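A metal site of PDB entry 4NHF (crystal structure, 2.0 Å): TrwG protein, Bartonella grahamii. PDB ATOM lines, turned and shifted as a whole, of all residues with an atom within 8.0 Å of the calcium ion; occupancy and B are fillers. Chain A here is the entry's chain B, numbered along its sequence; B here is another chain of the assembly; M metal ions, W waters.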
ATOM      1  N   TYR A  59      22.503  -8.514  18.360  1.00  0.00           N
ATOM      2  CA  TYR A  59      22.832  -8.489  16.970  1.00  0.00           C
ATOM      3  C   TYR A  59      22.380  -7.167  16.364  1.00  0.00           C
ATOM      4  O   TYR A  59      21.223  -6.754  16.548  1.00  0.00           O
ATOM      5  CB  TYR A  59      22.188  -9.626  16.149  1.00  0.00           C
ATOM      6  CG  TYR A  59      22.617  -9.496  14.738  1.00  0.00           C
ATOM      7  CD1 TYR A  59      23.859  -9.945  14.363  1.00  0.00           C
ATOM      8  CD2 TYR A  59      21.811  -8.851  13.771  1.00  0.00           C
ATOM      9  CE1 TYR A  59      24.312  -9.786  13.074  1.00  0.00           C
ATOM     10  CE2 TYR A  59      22.254  -8.700  12.487  1.00  0.00           C
ATOM     11  CZ  TYR A  59      23.494  -9.170  12.133  1.00  0.00           C
ATOM     12  OH  TYR A  59      23.964  -9.045  10.839  1.00  0.00           O
ATOM     13  N   ASP A  60      23.352  -6.491  15.759  1.00  0.00           N
ATOM     14  CA  ASP A  60      23.201  -5.193  15.102  1.00  0.00           C
ATOM     15  C   ASP A  60      24.313  -5.193  14.061  1.00  0.00           C
ATOM     16  O   ASP A  60      25.524  -5.196  14.394  1.00  0.00           O
ATOM     17  CB  ASP A  60      23.396  -4.063  16.123  1.00  0.00           C
ATOM     18  CG  ASP A  60      23.174  -2.685  15.560  1.00  0.00           C
ATOM     19  OD1 ASP A  60      23.175  -2.482  14.290  1.00  0.00           O
ATOM     20  OD2 ASP A  60      23.001  -1.774  16.441  1.00  0.00           O
ATOM     21  N   TYR A  61      23.923  -5.149  12.784  1.00  0.00           N
ATOM     22  CA  TYR A  61      24.894  -5.152  11.713  1.00  0.00           C
ATOM     23  C   TYR A  61      25.958  -4.121  11.914  1.00  0.00           C
ATOM     24  O   TYR A  61      27.109  -4.361  11.572  1.00  0.00           O
ATOM     25  CB  TYR A  61      24.222  -4.887  10.342  1.00  0.00           C
ATOM     26  CG  TYR A  61      25.164  -4.826   9.157  1.00  0.00           C
ATOM     27  CD1 TYR A  61      25.619  -5.978   8.522  1.00  0.00           C
ATOM     28  CD2 TYR A  61      25.566  -3.620   8.647  1.00  0.00           C
ATOM     29  CE1 TYR A  61      26.437  -5.896   7.383  1.00  0.00           C
ATOM     30  CE2 TYR A  61      26.374  -3.518   7.542  1.00  0.00           C
ATOM     31  CZ  TYR A  61      26.821  -4.669   6.912  1.00  0.00           C
ATOM     32  OH  TYR A  61      27.623  -4.494   5.800  1.00  0.00           O
ATOM     33  N   ASP A  62      25.594  -2.950  12.446  1.00  0.00           N
ATOM     34  CA  ASP A  62      26.557  -1.876  12.575  1.00  0.00           C
ATOM     35  C   ASP A  62      27.574  -2.059  13.682  1.00  0.00           C
ATOM     36  O   ASP A  62      28.616  -1.379  13.656  1.00  0.00           O
ATOM     37  CB  ASP A  62      25.864  -0.552  12.757  1.00  0.00           C
ATOM     38  CG  ASP A  62      24.927  -0.248  11.597  1.00  0.00           C
ATOM     39  OD1 ASP A  62      25.388  -0.231  10.446  1.00  0.00           O
ATOM     40  OD2 ASP A  62      23.716  -0.085  11.867  1.00  0.00           O
ATOM     41  N   THR A  63      27.290  -2.935  14.642  1.00  0.00           N
ATOM     42  CA  THR A  63      28.201  -3.201  15.753  1.00  0.00           C
ATOM     43  C   THR A  63      28.761  -4.636  15.816  1.00  0.00           C
ATOM     44  O   THR A  63      29.407  -5.008  16.825  1.00  0.00           O
ATOM     45  CB  THR A  63      27.581  -2.812  17.101  1.00  0.00           C
ATOM     46  OG1 THR A  63      26.519  -3.690  17.452  1.00  0.00           O
ATOM     47  CG2 THR A  63      27.096  -1.396  17.119  1.00  0.00           C
ATOM     48  N   ASN A  99      21.572  -6.471   7.541  1.00  0.00           N
ATOM     49  CA  ASN A  99      21.038  -5.329   8.261  1.00  0.00           C
ATOM     50  C   ASN A  99      19.509  -5.181   8.071  1.00  0.00           C
ATOM     51  O   ASN A  99      18.981  -4.059   8.017  1.00  0.00           O
ATOM     52  CB  ASN A  99      21.784  -4.052   7.869  1.00  0.00           C
ATOM     53  CG  ASN A  99      21.626  -2.938   8.908  1.00  0.00           C
ATOM     54  OD1 ASN A  99      21.256  -3.197  10.054  1.00  0.00           O
ATOM     55  ND2 ASN A  99      21.934  -1.732   8.529  1.00  0.00           N
ATOM     56  N   ALA A 101      17.493  -6.869  10.274  1.00  0.00           N
ATOM     57  CA  ALA A 101      16.931  -7.099  11.560  1.00  0.00           C
ATOM     58  C   ALA A 101      18.015  -6.946  12.635  1.00  0.00           C
ATOM     59  O   ALA A 101      19.222  -6.996  12.352  1.00  0.00           O
ATOM     60  CB  ALA A 101      16.306  -8.512  11.600  1.00  0.00           C
ATOM     61  N   ARG A 102      17.582  -6.646  13.848  1.00  0.00           N
ATOM     62  CA  ARG A 102      18.502  -6.581  15.024  1.00  0.00           C
ATOM     63  C   ARG A 102      17.983  -7.530  16.084  1.00  0.00           C
ATOM     64  O   ARG A 102      16.818  -7.908  16.038  1.00  0.00           O
ATOM     65  CB  ARG A 102      18.500  -5.187  15.630  1.00  0.00           C
ATOM     66  CG  ARG A 102      19.182  -4.098  14.802  1.00  0.00           C
ATOM     67  CD  ARG A 102      19.183  -2.767  15.611  1.00  0.00           C
ATOM     68  NE  ARG A 102      17.912  -2.125  15.368  1.00  0.00           N
ATOM     69  CZ  ARG A 102      17.342  -1.170  16.077  1.00  0.00           C
ATOM     70  NH1 ARG A 102      17.919  -0.687  17.149  1.00  0.00           N
ATOM     71  NH2 ARG A 102      16.147  -0.686  15.675  1.00  0.00           N
ATOM     72  N   SER A 129      13.583  -1.678  11.824  1.00  0.00           N
ATOM     73  CA  SER A 129      14.336  -0.443  11.983  1.00  0.00           C
ATOM     74  C   SER A 129      13.567   0.456  12.916  1.00  0.00           C
ATOM     75  O   SER A 129      14.084   1.467  13.317  1.00  0.00           O
ATOM     76  CB  SER A 129      14.532   0.247  10.639  1.00  0.00           C
ATOM     77  OG  SER A 129      13.304   0.355   9.964  1.00  0.00           O
ATOM     78  N   ASP B  60      25.020   7.189  17.204  1.00  0.00           N
ATOM     79  CA  ASP B  60      24.355   6.124  16.445  1.00  0.00           C
ATOM     80  C   ASP B  60      22.941   6.159  16.965  1.00  0.00           C
ATOM     81  O   ASP B  60      22.714   5.912  18.143  1.00  0.00           O
ATOM     82  CB  ASP B  60      25.012   4.761  16.711  1.00  0.00           C
ATOM     83  CG  ASP B  60      24.454   3.612  15.821  1.00  0.00           C
ATOM     84  OD1 ASP B  60      23.284   3.707  15.346  1.00  0.00           O
ATOM     85  OD2 ASP B  60      25.179   2.565  15.680  1.00  0.00           O
ATOM     86  N   TYR B  61      21.975   6.492  16.104  1.00  0.00           N
ATOM     87  CA  TYR B  61      20.578   6.571  16.513  1.00  0.00           C
ATOM     88  C   TYR B  61      20.161   5.292  17.294  1.00  0.00           C
ATOM     89  O   TYR B  61      19.396   5.332  18.266  1.00  0.00           O
ATOM     90  CB  TYR B  61      19.681   6.760  15.260  1.00  0.00           C
ATOM     91  CG  TYR B  61      18.229   6.947  15.579  1.00  0.00           C
ATOM     92  CD1 TYR B  61      17.783   8.130  16.166  1.00  0.00           C
ATOM     93  CD2 TYR B  61      17.308   5.941  15.351  1.00  0.00           C
ATOM     94  CE1 TYR B  61      16.444   8.304  16.495  1.00  0.00           C
ATOM     95  CE2 TYR B  61      15.971   6.094  15.687  1.00  0.00           C
ATOM     96  CZ  TYR B  61      15.557   7.282  16.267  1.00  0.00           C
ATOM     97  OH  TYR B  61      14.225   7.465  16.605  1.00  0.00           O
ATOM     98  N   ASP B  62      20.669   4.139  16.866  1.00  0.00           N
ATOM     99  CA  ASP B  62      20.190   2.875  17.402  1.00  0.00           C
ATOM    100  C   ASP B  62      20.808   2.658  18.827  1.00  0.00           C
ATOM    101  O   ASP B  62      20.256   1.925  19.587  1.00  0.00           O
ATOM    102  CB  ASP B  62      20.629   1.731  16.503  1.00  0.00           C
ATOM    103  CG  ASP B  62      19.820   1.608  15.234  1.00  0.00           C
ATOM    104  OD1 ASP B  62      18.866   2.402  15.033  1.00  0.00           O
ATOM    105  OD2 ASP B  62      20.132   0.633  14.470  1.00  0.00           O
ATOM    106  N   THR B  63      21.883   3.321  19.184  1.00  0.00           N
ATOM    107  CA  THR B  63      22.455   3.119  20.498  1.00  0.00           C
ATOM    108  C   THR B  63      22.501   4.398  21.351  1.00  0.00           C
ATOM    109  O   THR B  63      23.208   4.443  22.336  1.00  0.00           O
ATOM    110  CB  THR B  63      23.858   2.491  20.407  1.00  0.00           C
ATOM    111  OG1 THR B  63      24.793   3.387  19.804  1.00  0.00           O
ATOM    112  CG2 THR B  63      23.851   1.219  19.649  1.00  0.00           C
ATOM    113  N   ARG B 102      25.617   9.135  11.350  1.00  0.00           N
ATOM    114  CA  ARG B 102      26.376   8.573  12.446  1.00  0.00           C
ATOM    115  C   ARG B 102      27.674   9.347  12.621  1.00  0.00           C
ATOM    116  O   ARG B 102      28.130  10.015  11.695  1.00  0.00           O
ATOM    117  CB  ARG B 102      26.660   7.086  12.196  1.00  0.00           C
ATOM    118  CG  ARG B 102      25.525   6.155  12.632  1.00  0.00           C
ATOM    119  CD  ARG B 102      25.050   5.227  11.525  1.00  0.00           C
ATOM    120  NE  ARG B 102      26.086   4.357  10.990  1.00  0.00           N
ATOM    121  CZ  ARG B 102      26.686   3.427  11.727  1.00  0.00           C
ATOM    122  NH1 ARG B 102      27.638   2.664  11.205  1.00  0.00           N
ATOM    123  NH2 ARG B 102      26.334   3.280  13.002  1.00  0.00           N
HETATM  124 CA    CA M   1      22.160  -0.208  13.527  1.00  0.00          CA
HETATM  125  O   HOH W   1      20.730  -1.622  12.293  1.00  0.00           O
HETATM  126  O   HOH W   2      23.636   0.398  15.546  1.00  0.00           O
HETATM  127  O   HOH W   3      22.859   2.043  13.552  1.00  0.00           O
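The side-chain carboxylate (OD1) of Asp 62 of chain A is in salt-bridge range of the guanidinium group (NH1) of Arg 102 of chain B, 3.7 Å away. OD1 of Asp 62 of chain B is in salt-bridge range of NH1 of Arg 102 of chain A (3.9 Å). The backbone NH of Asp 62 of chain B lies close to the side-chain carboxylate of Asp 60 of chain B, 3.1 Å away.
Of the 14 residues printed, 3 come within 4 Å of the calcium ion. Along chain A the residues within 4 Å of the calcium ion span positions 60 to 62.
The calcium ion is bound by OD2 of Asp 62 of chain A, water W3, water W1, OD2 of Asp 62 of chain B, water W2 and OD1 of Asp 60 of chain A.
Water W2 lies within hydrogen-bond range of OD2 of Asp 60 of chain A (2.4 Å) and OD2 of Asp 60 of chain B (2.7 Å).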
